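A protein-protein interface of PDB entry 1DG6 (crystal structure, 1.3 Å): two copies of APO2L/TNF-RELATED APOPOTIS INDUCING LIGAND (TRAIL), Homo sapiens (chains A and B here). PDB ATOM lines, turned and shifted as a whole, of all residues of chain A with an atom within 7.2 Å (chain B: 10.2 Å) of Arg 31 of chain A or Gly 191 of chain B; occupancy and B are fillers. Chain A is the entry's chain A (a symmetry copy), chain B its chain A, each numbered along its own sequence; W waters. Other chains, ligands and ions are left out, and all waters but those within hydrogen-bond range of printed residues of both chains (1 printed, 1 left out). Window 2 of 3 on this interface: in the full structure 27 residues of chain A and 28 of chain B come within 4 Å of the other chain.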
ATOM      1  N   GLN A  30      30.183 -30.895   6.618  1.00  0.00           N
ATOM      2  CA  GLN A  30      29.290 -29.817   6.183  1.00  0.00           C
ATOM      3  C   GLN A  30      30.025 -28.754   5.388  1.00  0.00           C
ATOM      4  O   GLN A  30      30.978 -28.130   5.841  1.00  0.00           O
ATOM      5  CB  GLN A  30      28.625 -29.210   7.426  1.00  0.00           C
ATOM      6  CG  GLN A  30      29.620 -28.857   8.516  1.00  0.00           C
ATOM      7  CD  GLN A  30      29.682 -27.355   8.754  1.00  0.00           C
ATOM      8  OE1 GLN A  30      29.528 -26.908   9.901  1.00  0.00           O
ATOM      9  NE2 GLN A  30      29.915 -26.637   7.656  1.00  0.00           N
ATOM     10  N   ARG A  31      29.615 -28.496   4.154  1.00  0.00           N
ATOM     11  CA  ARG A  31      30.298 -27.578   3.270  1.00  0.00           C
ATOM     12  C   ARG A  31      31.797 -27.920   3.187  1.00  0.00           C
ATOM     13  O   ARG A  31      32.676 -27.216   3.679  1.00  0.00           O
ATOM     14  CB  ARG A  31      30.115 -26.113   3.630  1.00  0.00           C
ATOM     15  CG  ARG A  31      28.690 -25.807   4.062  1.00  0.00           C
ATOM     16  CD  ARG A  31      28.383 -24.316   3.980  1.00  0.00           C
ATOM     17  NE  ARG A  31      27.882 -23.877   2.685  1.00  0.00           N
ATOM     18  CZ  ARG A  31      28.125 -22.688   2.154  1.00  0.00           C
ATOM     19  NH1 ARG A  31      28.878 -21.860   2.859  1.00  0.00           N
ATOM     20  NH2 ARG A  31      27.604 -22.403   0.970  1.00  0.00           N
ATOM     21  N   VAL A  32      32.020 -29.028   2.524  1.00  0.00           N
ATOM     22  CA  VAL A  32      33.355 -29.450   2.129  1.00  0.00           C
ATOM     23  C   VAL A  32      33.409 -29.410   0.609  1.00  0.00           C
ATOM     24  O   VAL A  32      32.842 -30.295  -0.052  1.00  0.00           O
ATOM     25  CB  VAL A  32      33.637 -30.851   2.712  1.00  0.00           C
ATOM     26  CG1 VAL A  32      35.081 -31.216   2.365  1.00  0.00           C
ATOM     27  CG2 VAL A  32      33.427 -30.920   4.216  1.00  0.00           C
ATOM     28  N   ALA A  33      34.016 -28.356   0.063  1.00  0.00           N
ATOM     29  CA  ALA A  33      34.022 -28.138  -1.387  1.00  0.00           C
ATOM     30  C   ALA A  33      35.078 -27.116  -1.769  1.00  0.00           C
ATOM     31  O   ALA A  33      35.481 -26.310  -0.956  1.00  0.00           O
ATOM     32  CB  ALA A  33      32.635 -27.667  -1.848  1.00  0.00           C
ATOM     33  N   PHE A  73      36.992 -20.499  -4.577  1.00  0.00           N
ATOM     34  CA  PHE A  73      36.800 -20.617  -3.135  1.00  0.00           C
ATOM     35  C   PHE A  73      37.317 -21.957  -2.625  1.00  0.00           C
ATOM     36  O   PHE A  73      37.430 -22.918  -3.414  1.00  0.00           O
ATOM     37  CB  PHE A  73      35.319 -20.479  -2.743  1.00  0.00           C
ATOM     38  CG  PHE A  73      34.464 -21.708  -3.055  1.00  0.00           C
ATOM     39  CD1 PHE A  73      33.921 -21.912  -4.329  1.00  0.00           C
ATOM     40  CD2 PHE A  73      34.175 -22.675  -2.098  1.00  0.00           C
ATOM     41  CE1 PHE A  73      33.168 -23.054  -4.612  1.00  0.00           C
ATOM     42  CE2 PHE A  73      33.464 -23.814  -2.384  1.00  0.00           C
ATOM     43  CZ  PHE A  73      32.933 -24.017  -3.655  1.00  0.00           C
ATOM     44  N   LEU A  74      37.567 -21.950  -1.319  1.00  0.00           N
ATOM     45  CA  LEU A  74      37.933 -23.196  -0.637  1.00  0.00           C
ATOM     46  C   LEU A  74      37.079 -23.351   0.590  1.00  0.00           C
ATOM     47  O   LEU A  74      36.918 -22.336   1.335  1.00  0.00           O
ATOM     48  CB  LEU A  74      39.418 -23.149  -0.252  1.00  0.00           C
ATOM     49  CG  LEU A  74      40.391 -23.082  -1.432  1.00  0.00           C
ATOM     50  CD1 LEU A  74      41.759 -22.537  -0.984  1.00  0.00           C
ATOM     51  CD2 LEU A  74      40.597 -24.446  -2.058  1.00  0.00           C
ATOM     52  N   SER A  75      36.567 -24.520   0.896  1.00  0.00           N
ATOM     53  CA  SER A  75      35.757 -24.694   2.121  1.00  0.00           C
ATOM     54  C   SER A  75      36.120 -26.033   2.720  1.00  0.00           C
ATOM     55  O   SER A  75      35.717 -27.084   2.183  1.00  0.00           O
ATOM     56  CB  SER A  75      34.273 -24.573   1.806  1.00  0.00           C
ATOM     57  OG  SER A  75      33.461 -24.666   3.002  1.00  0.00           O
ATOM     58  N   ASN A  76      36.896 -26.002   3.810  1.00  0.00           N
ATOM     59  CA  ASN A  76      37.322 -27.253   4.472  1.00  0.00           C
ATOM     60  C   ASN A  76      38.218 -28.127   3.563  1.00  0.00           C
ATOM     61  O   ASN A  76      38.281 -29.347   3.752  1.00  0.00           O
ATOM     62  CB  ASN A  76      36.156 -28.078   5.003  1.00  0.00           C
ATOM     63  CG  ASN A  76      35.531 -27.514   6.264  1.00  0.00           C
ATOM     64  OD1 ASN A  76      36.189 -27.441   7.316  1.00  0.00           O
ATOM     65  ND2 ASN A  76      34.250 -27.112   6.201  1.00  0.00           N
ATOM     66  N   LEU A  77      38.915 -27.457   2.681  1.00  0.00           N
ATOM     67  CA  LEU A  77      40.035 -27.927   1.903  1.00  0.00           C
ATOM     68  C   LEU A  77      41.036 -26.784   1.869  1.00  0.00           C
ATOM     69  O   LEU A  77      40.617 -25.625   2.091  1.00  0.00           O
ATOM     70  CB  LEU A  77      39.652 -28.272   0.432  1.00  0.00           C
ATOM     71  CG  LEU A  77      38.901 -29.553   0.117  1.00  0.00           C
ATOM     72  CD1 LEU A  77      37.424 -29.316   0.088  1.00  0.00           C
ATOM     73  CD2 LEU A  77      39.301 -30.125  -1.256  1.00  0.00           C
ATOM     74  N   PHE A 188      34.145 -31.877  -4.341  1.00  0.00           N
ATOM     75  CA  PHE A 188      33.221 -31.722  -3.226  1.00  0.00           C
ATOM     76  C   PHE A 188      32.959 -33.095  -2.621  1.00  0.00           C
ATOM     77  O   PHE A 188      33.007 -34.102  -3.283  1.00  0.00           O
ATOM     78  CB  PHE A 188      31.878 -31.079  -3.591  1.00  0.00           C
ATOM     79  CG  PHE A 188      31.068 -31.734  -4.704  1.00  0.00           C
ATOM     80  CD1 PHE A 188      31.282 -31.377  -6.057  1.00  0.00           C
ATOM     81  CD2 PHE A 188      30.094 -32.664  -4.414  1.00  0.00           C
ATOM     82  CE1 PHE A 188      30.512 -31.961  -7.056  1.00  0.00           C
ATOM     83  CE2 PHE A 188      29.344 -33.316  -5.415  1.00  0.00           C
ATOM     84  CZ  PHE A 188      29.594 -32.934  -6.723  1.00  0.00           C
ATOM     85  N   LEU A 189      32.682 -33.024  -1.306  1.00  0.00           N
ATOM     86  CA  LEU A 189      32.419 -34.273  -0.553  1.00  0.00           C
ATOM     87  C   LEU A 189      31.025 -34.776  -0.855  1.00  0.00           C
ATOM     88  O   LEU A 189      30.047 -34.016  -0.767  1.00  0.00           O
ATOM     89  CB  LEU A 189      32.617 -33.924   0.913  1.00  0.00           C
ATOM     90  CG  LEU A 189      32.414 -35.069   1.902  1.00  0.00           C
ATOM     91  CD1 LEU A 189      33.505 -36.113   1.733  1.00  0.00           C
ATOM     92  CD2 LEU A 189      32.388 -34.498   3.320  1.00  0.00           C
ATOM     93  N   GLN B  30      17.224 -29.651   1.581  1.00  0.00           N
ATOM     94  CA  GLN B  30      16.881 -31.040   1.263  1.00  0.00           C
ATOM     95  C   GLN B  30      16.257 -31.173  -0.113  1.00  0.00           C
ATOM     96  O   GLN B  30      15.236 -30.576  -0.436  1.00  0.00           O
ATOM     97  CB  GLN B  30      15.932 -31.564   2.349  1.00  0.00           C
ATOM     98  CG  GLN B  30      14.765 -30.630   2.614  1.00  0.00           C
ATOM     99  CD  GLN B  30      13.438 -31.263   2.221  1.00  0.00           C
ATOM    100  OE1 GLN B  30      12.512 -31.309   3.046  1.00  0.00           O
ATOM    101  NE2 GLN B  30      13.399 -31.718   0.970  1.00  0.00           N
ATOM    102  N   VAL B  32      17.425 -30.146  -3.250  1.00  0.00           N
ATOM    103  CA  VAL B  32      17.570 -28.938  -4.047  1.00  0.00           C
ATOM    104  C   VAL B  32      18.346 -29.316  -5.300  1.00  0.00           C
ATOM    105  O   VAL B  32      19.569 -29.517  -5.232  1.00  0.00           O
ATOM    106  CB  VAL B  32      18.270 -27.853  -3.201  1.00  0.00           C
ATOM    107  CG1 VAL B  32      18.310 -26.571  -4.033  1.00  0.00           C
ATOM    108  CG2 VAL B  32      17.572 -27.594  -1.875  1.00  0.00           C
ATOM    109  N   ILE B  86      17.344 -19.514  -8.317  1.00  0.00           N
ATOM    110  CA  ILE B  86      17.744 -20.122  -7.070  1.00  0.00           C
ATOM    111  C   ILE B  86      16.853 -19.656  -5.926  1.00  0.00           C
ATOM    112  O   ILE B  86      16.558 -18.467  -5.734  1.00  0.00           O
ATOM    113  CB  ILE B  86      19.228 -19.738  -6.773  1.00  0.00           C
ATOM    114  CG1 ILE B  86      20.164 -20.141  -7.923  1.00  0.00           C
ATOM    115  CG2 ILE B  86      19.741 -20.281  -5.433  1.00  0.00           C
ATOM    116  CD1 ILE B  86      20.079 -21.567  -8.392  1.00  0.00           C
ATOM    117  N   GLU B  88      17.484 -21.222  -2.594  1.00  0.00           N
ATOM    118  CA  GLU B  88      18.282 -21.422  -1.382  1.00  0.00           C
ATOM    119  C   GLU B  88      19.748 -21.076  -1.600  1.00  0.00           C
ATOM    120  O   GLU B  88      20.368 -21.654  -2.527  1.00  0.00           O
ATOM    121  CB  GLU B  88      18.191 -22.906  -0.945  1.00  0.00           C
ATOM    122  CG  GLU B  88      16.725 -23.293  -0.660  1.00  0.00           C
ATOM    123  CD  GLU B  88      16.350 -22.640   0.663  1.00  0.00           C
ATOM    124  OE1 GLU B  88      17.115 -22.880   1.623  1.00  0.00           O
ATOM    125  OE2 GLU B  88      15.337 -21.930   0.709  1.00  0.00           O
ATOM    126  N   LYS B  89      20.335 -20.190  -0.810  1.00  0.00           N
ATOM    127  CA  LYS B  89      21.745 -19.845  -0.996  1.00  0.00           C
ATOM    128  C   LYS B  89      22.614 -21.058  -0.718  1.00  0.00           C
ATOM    129  O   LYS B  89      22.323 -21.935   0.149  1.00  0.00           O
ATOM    130  CB  LYS B  89      22.125 -18.629  -0.119  1.00  0.00           C
ATOM    131  CG  LYS B  89      22.113 -18.957   1.371  1.00  0.00           C
ATOM    132  CD  LYS B  89      22.714 -17.837   2.215  1.00  0.00           C
ATOM    133  CE  LYS B  89      23.153 -18.361   3.577  1.00  0.00           C
ATOM    134  NZ  LYS B  89      22.755 -17.448   4.691  1.00  0.00           N
ATOM    135  N   GLY B  90      23.749 -21.184  -1.427  1.00  0.00           N
ATOM    136  CA  GLY B  90      24.697 -22.259  -1.119  1.00  0.00           C
ATOM    137  C   GLY B  90      25.605 -22.559  -2.309  1.00  0.00           C
ATOM    138  O   GLY B  90      25.578 -21.794  -3.303  1.00  0.00           O
ATOM    139  N   PHE B  91      26.374 -23.631  -2.145  1.00  0.00           N
ATOM    140  CA  PHE B  91      27.292 -24.055  -3.205  1.00  0.00           C
ATOM    141  C   PHE B  91      26.522 -24.935  -4.187  1.00  0.00           C
ATOM    142  O   PHE B  91      25.917 -25.916  -3.695  1.00  0.00           O
ATOM    143  CB  PHE B  91      28.479 -24.846  -2.622  1.00  0.00           C
ATOM    144  CG  PHE B  91      29.357 -24.066  -1.697  1.00  0.00           C
ATOM    145  CD1 PHE B  91      29.814 -22.800  -2.033  1.00  0.00           C
ATOM    146  CD2 PHE B  91      29.754 -24.624  -0.493  1.00  0.00           C
ATOM    147  CE1 PHE B  91      30.631 -22.135  -1.128  1.00  0.00           C
ATOM    148  CE2 PHE B  91      30.596 -23.995   0.410  1.00  0.00           C
ATOM    149  CZ  PHE B  91      30.993 -22.702   0.081  1.00  0.00           C
ATOM    150  N   TYR B  92      26.530 -24.632  -5.476  1.00  0.00           N
ATOM    151  CA  TYR B  92      25.829 -25.479  -6.443  1.00  0.00           C
ATOM    152  C   TYR B  92      26.825 -26.040  -7.466  1.00  0.00           C
ATOM    153  O   TYR B  92      27.583 -25.245  -8.021  1.00  0.00           O
ATOM    154  CB  TYR B  92      24.782 -24.703  -7.229  1.00  0.00           C
ATOM    155  CG  TYR B  92      23.557 -24.387  -6.400  1.00  0.00           C
ATOM    156  CD1 TYR B  92      23.571 -23.365  -5.445  1.00  0.00           C
ATOM    157  CD2 TYR B  92      22.389 -25.156  -6.587  1.00  0.00           C
ATOM    158  CE1 TYR B  92      22.421 -23.116  -4.696  1.00  0.00           C
ATOM    159  CE2 TYR B  92      21.251 -24.905  -5.839  1.00  0.00           C
ATOM    160  CZ  TYR B  92      21.275 -23.878  -4.899  1.00  0.00           C
ATOM    161  OH  TYR B  92      20.105 -23.663  -4.170  1.00  0.00           O
ATOM    162  N   TYR B  93      26.741 -27.347  -7.728  1.00  0.00           N
ATOM    163  CA  TYR B  93      27.366 -27.855  -8.941  1.00  0.00           C
ATOM    164  C   TYR B  93      26.401 -27.593 -10.091  1.00  0.00           C
ATOM    165  O   TYR B  93      25.236 -28.035 -10.045  1.00  0.00           O
ATOM    166  CB  TYR B  93      27.673 -29.369  -8.757  1.00  0.00           C
ATOM    167  CG  TYR B  93      28.339 -29.887 -10.019  1.00  0.00           C
ATOM    168  CD1 TYR B  93      29.706 -29.795 -10.224  1.00  0.00           C
ATOM    169  CD2 TYR B  93      27.582 -30.505 -11.035  1.00  0.00           C
ATOM    170  CE1 TYR B  93      30.306 -30.274 -11.380  1.00  0.00           C
ATOM    171  CE2 TYR B  93      28.182 -30.999 -12.196  1.00  0.00           C
ATOM    172  CZ  TYR B  93      29.561 -30.882 -12.363  1.00  0.00           C
ATOM    173  OH  TYR B  93      30.070 -31.348 -13.554  1.00  0.00           O
ATOM    174  N   ILE B 157      31.493 -25.946  -9.485  1.00  0.00           N
ATOM    175  CA  ILE B 157      30.768 -25.530  -8.299  1.00  0.00           C
ATOM    176  C   ILE B 157      30.910 -24.036  -8.060  1.00  0.00           C
ATOM    177  O   ILE B 157      32.036 -23.524  -8.120  1.00  0.00           O
ATOM    178  CB  ILE B 157      31.331 -26.228  -7.036  1.00  0.00           C
ATOM    179  CG1 ILE B 157      31.508 -27.712  -7.129  1.00  0.00           C
ATOM    180  CG2 ILE B 157      30.422 -25.825  -5.847  1.00  0.00           C
ATOM    181  CD1 ILE B 157      32.585 -28.178  -6.151  1.00  0.00           C
ATOM    182  N   PHE B 158      29.770 -23.365  -7.835  1.00  0.00           N
ATOM    183  CA  PHE B 158      29.711 -21.919  -7.625  1.00  0.00           C
ATOM    184  C   PHE B 158      28.818 -21.576  -6.454  1.00  0.00           C
ATOM    185  O   PHE B 158      27.772 -22.222  -6.228  1.00  0.00           O
ATOM    186  CB  PHE B 158      29.181 -21.209  -8.917  1.00  0.00           C
ATOM    187  CG  PHE B 158      30.168 -21.383 -10.066  1.00  0.00           C
ATOM    188  CD1 PHE B 158      30.116 -22.554 -10.845  1.00  0.00           C
ATOM    189  CD2 PHE B 158      31.170 -20.451 -10.300  1.00  0.00           C
ATOM    190  CE1 PHE B 158      31.088 -22.790 -11.804  1.00  0.00           C
ATOM    191  CE2 PHE B 158      32.119 -20.658 -11.310  1.00  0.00           C
ATOM    192  CZ  PHE B 158      32.096 -21.843 -12.039  1.00  0.00           C
ATOM    193  N   GLU B 159      29.236 -20.520  -5.730  1.00  0.00           N
ATOM    194  CA  GLU B 159      28.366 -20.020  -4.646  1.00  0.00           C
ATOM    195  C   GLU B 159      27.278 -19.160  -5.219  1.00  0.00           C
ATOM    196  O   GLU B 159      27.546 -18.173  -5.921  1.00  0.00           O
ATOM    197  CB  GLU B 159      29.165 -19.216  -3.613  1.00  0.00           C
ATOM    198  CG  GLU B 159      28.211 -18.952  -2.429  1.00  0.00           C
ATOM    199  CD  GLU B 159      28.756 -19.346  -1.084  1.00  0.00           C
ATOM    200  OE1 GLU B 159      29.777 -18.780  -0.607  1.00  0.00           O
ATOM    201  OE2 GLU B 159      28.186 -20.265  -0.426  1.00  0.00           O
ATOM    202  N   LEU B 160      26.031 -19.522  -4.933  1.00  0.00           N
ATOM    203  CA  LEU B 160      24.912 -18.749  -5.451  1.00  0.00           C
ATOM    204  C   LEU B 160      24.040 -18.213  -4.311  1.00  0.00           C
ATOM    205  O   LEU B 160      23.995 -18.810  -3.229  1.00  0.00           O
ATOM    206  CB  LEU B 160      24.024 -19.585  -6.379  1.00  0.00           C
ATOM    207  CG  LEU B 160      24.704 -20.276  -7.561  1.00  0.00           C
ATOM    208  CD1 LEU B 160      23.709 -21.131  -8.347  1.00  0.00           C
ATOM    209  CD2 LEU B 160      25.339 -19.210  -8.457  1.00  0.00           C
ATOM    210  N   LYS B 161      23.404 -17.087  -4.581  1.00  0.00           N
ATOM    211  CA  LYS B 161      22.528 -16.444  -3.597  1.00  0.00           C
ATOM    212  C   LYS B 161      21.072 -16.670  -3.980  1.00  0.00           C
ATOM    213  O   LYS B 161      20.770 -16.893  -5.149  1.00  0.00           O
ATOM    214  CB  LYS B 161      22.803 -14.917  -3.547  1.00  0.00           C
ATOM    215  CG  LYS B 161      24.223 -14.554  -3.070  1.00  0.00           C
ATOM    216  CD  LYS B 161      24.290 -13.042  -2.884  1.00  0.00           C
ATOM    217  CE  LYS B 161      25.640 -12.497  -2.519  1.00  0.00           C
ATOM    218  NZ  LYS B 161      26.479 -13.469  -1.792  1.00  0.00           N
ATOM    219  N   ALA B 187      21.559 -28.383 -12.082  1.00  0.00           N
ATOM    220  CA  ALA B 187      22.328 -27.936 -10.940  1.00  0.00           C
ATOM    221  C   ALA B 187      21.873 -28.662  -9.684  1.00  0.00           C
ATOM    222  O   ALA B 187      20.683 -29.033  -9.614  1.00  0.00           O
ATOM    223  CB  ALA B 187      22.144 -26.435 -10.751  1.00  0.00           C
ATOM    224  N   PHE B 188      22.743 -28.788  -8.694  1.00  0.00           N
ATOM    225  CA  PHE B 188      22.294 -29.332  -7.420  1.00  0.00           C
ATOM    226  C   PHE B 188      23.124 -28.706  -6.306  1.00  0.00           C
ATOM    227  O   PHE B 188      24.258 -28.340  -6.487  1.00  0.00           O
ATOM    228  CB  PHE B 188      22.391 -30.859  -7.307  1.00  0.00           C
ATOM    229  CG  PHE B 188      23.751 -31.495  -7.567  1.00  0.00           C
ATOM    230  CD1 PHE B 188      24.139 -31.855  -8.880  1.00  0.00           C
ATOM    231  CD2 PHE B 188      24.616 -31.761  -6.528  1.00  0.00           C
ATOM    232  CE1 PHE B 188      25.369 -32.465  -9.094  1.00  0.00           C
ATOM    233  CE2 PHE B 188      25.895 -32.321  -6.729  1.00  0.00           C
ATOM    234  CZ  PHE B 188      26.228 -32.650  -8.033  1.00  0.00           C
ATOM    235  N   LEU B 189      22.439 -28.622  -5.151  1.00  0.00           N
ATOM    236  CA  LEU B 189      23.091 -28.019  -3.965  1.00  0.00           C
ATOM    237  C   LEU B 189      24.068 -28.999  -3.355  1.00  0.00           C
ATOM    238  O   LEU B 189      23.716 -30.162  -3.098  1.00  0.00           O
ATOM    239  CB  LEU B 189      21.964 -27.641  -3.018  1.00  0.00           C
ATOM    240  CG  LEU B 189      22.388 -26.977  -1.711  1.00  0.00           C
ATOM    241  CD1 LEU B 189      22.972 -25.601  -1.983  1.00  0.00           C
ATOM    242  CD2 LEU B 189      21.179 -26.908  -0.777  1.00  0.00           C
ATOM    243  N   VAL B 190      25.333 -28.558  -3.216  1.00  0.00           N
ATOM    244  CA  VAL B 190      26.318 -29.476  -2.660  1.00  0.00           C
ATOM    245  C   VAL B 190      26.471 -29.056  -1.198  1.00  0.00           C
ATOM    246  O   VAL B 190      26.776 -29.936  -0.419  1.00  0.00           O
ATOM    247  CB  VAL B 190      27.669 -29.634  -3.382  1.00  0.00           C
ATOM    248  CG1 VAL B 190      27.897 -28.917  -4.681  1.00  0.00           C
ATOM    249  CG2 VAL B 190      28.793 -29.279  -2.376  1.00  0.00           C
ATOM    250  N   GLY B 191      26.253 -27.809  -0.817  1.00  0.00           N
ATOM    251  CA  GLY B 191      26.201 -27.651   0.637  1.00  0.00           C
ATOM    252  C   GLY B 191      26.287 -26.177   0.974  1.00  0.00           C
ATOM    253  O   GLY B 191      26.678 -25.982   2.134  1.00  0.00           O
ATOM    254  OXT GLY B 191      25.995 -25.306   0.146  1.00  0.00           O
HETATM  255  O   HOH W   1      27.476 -29.582   2.319  1.00  0.00           O
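Phe 188 of chain B touches its own counterpart, Phe 188 of chain A.
Of the 11 pairs that touch across the chains among the printed residues, 1 has its exchanged pair printed and touching as well.
The side-chain carboxylate of Glu 159 of chain B lies within salt-bridge range of the guanidinium group of Arg 31 of chain A, 2.6 Å away.
The chain-end carboxylate (O) of Gly 191 of chain B lies within salt-bridge range of the guanidinium group (NE) of Arg 31 of chain A (2.5 Å).
Arg 31 of chain A touches just these residues of chain B: Gly 90 (3.6 Å), Phe 91 (3.3 Å), Glu 159 (2.6 Å) and Gly 191 (2.5 Å).
Of chain A, only Arg 31 (2.5 Å) comes within 4 Å of Gly 191 of chain B.
No residue of chain B comes within 4 Å of Gln 30 of chain A.
No residue of chain B comes within 4 Å of Val 32 of chain A.
Ser 75 of chain A touches just one residue of chain B: Phe 91 (3.9 Å).
Of the printed residues of chain A, Tyr 93 of chain B touches Phe 188.
Of the printed residues of chain B, Phe 73 of chain A touches Phe 91 and Ile 157.
Of the printed residues of chain A, Phe 188 of chain B touches Phe 188 (3.6 Å).
Printed residues of chain A within 4 Å of Val 190 of chain B: Phe 188.
Lys 161 of chain B touches none of the printed residues of chain A.
Leu 74 of chain A touches none of the printed residues of chain B.
O of Gly 90 of chain B is in hydrogen-bond range of N of Leu 160 of chain B.
The backbone carbonyl oxygen (O) of Phe 91 of chain B lies within hydrogen-bond range of the backbone NH (N) of Val 190 of chain B (2.7 Å).
O of Tyr 93 of chain B sits at hydrogen-bond distance from N of Phe 188 of chain B (2.9 Å).
OG of Ser 75 of chain A lies within hydrogen-bond range of O of Arg 31 of chain A (2.8 Å).
O of Arg 31 of chain A lies within hydrogen-bond range of ND2 of Asn 76 of chain A (3.0 Å).
The backbone carbonyl oxygen of Ala 33 of chain A sits at hydrogen-bond distance from the backbone NH of Ser 75 of chain A.
Printed residues of chain B that touch a printed residue of chain A: Gly 90, Phe 91, Tyr 93, Ile 157, Glu 159, Phe 188, Val 190 and Gly 191.
Hydrophobic or aromatic side chains of chain B that line the printed part of chain A: Phe 91, Tyr 93, Ile 157, Phe 188 and Val 190.
Of the 11 printed residues of chain A, 4 touch a printed residue of chain B.
Hydrophobic or aromatic side chains of chain A within 4 Å of the printed part of chain B: Phe 73 and Phe 188.
Among the printed residues, 11 pairs touch across the chains.
Gly 90 of chain B touches Arg 31 of chain A (CA to NH2, 3.6 Å).
CZ of Arg 31 of chain A touches CE2 of Phe 91 of chain B, 3.3 Å away.
Phe 91 of chain B touches Phe 73 of chain A.
Phe 73 of chain A touches Ile 157 of chain B (CE1 to O, 3.7 Å).
CE2 of Phe 91 of chain B touches OG of Ser 75 of chain A, 3.9 Å away.
Tyr 93 of chain B touches Phe 188 of chain A (CD1 to CE1, 3.9 Å).
Ile 157 of chain B touches Phe 188 of chain A (CD1 to CD1, 3.5 Å).
Phe 188 of chain A touches Phe 188 of chain B.
CB of Phe 188 of chain A touches CG2 of Val 190 of chain B, 3.8 Å away.
Water W1 lies within hydrogen-bond range of O of Val 190 of chain B (2.8 Å) and N of Arg 31 of chain A (3.0 Å).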
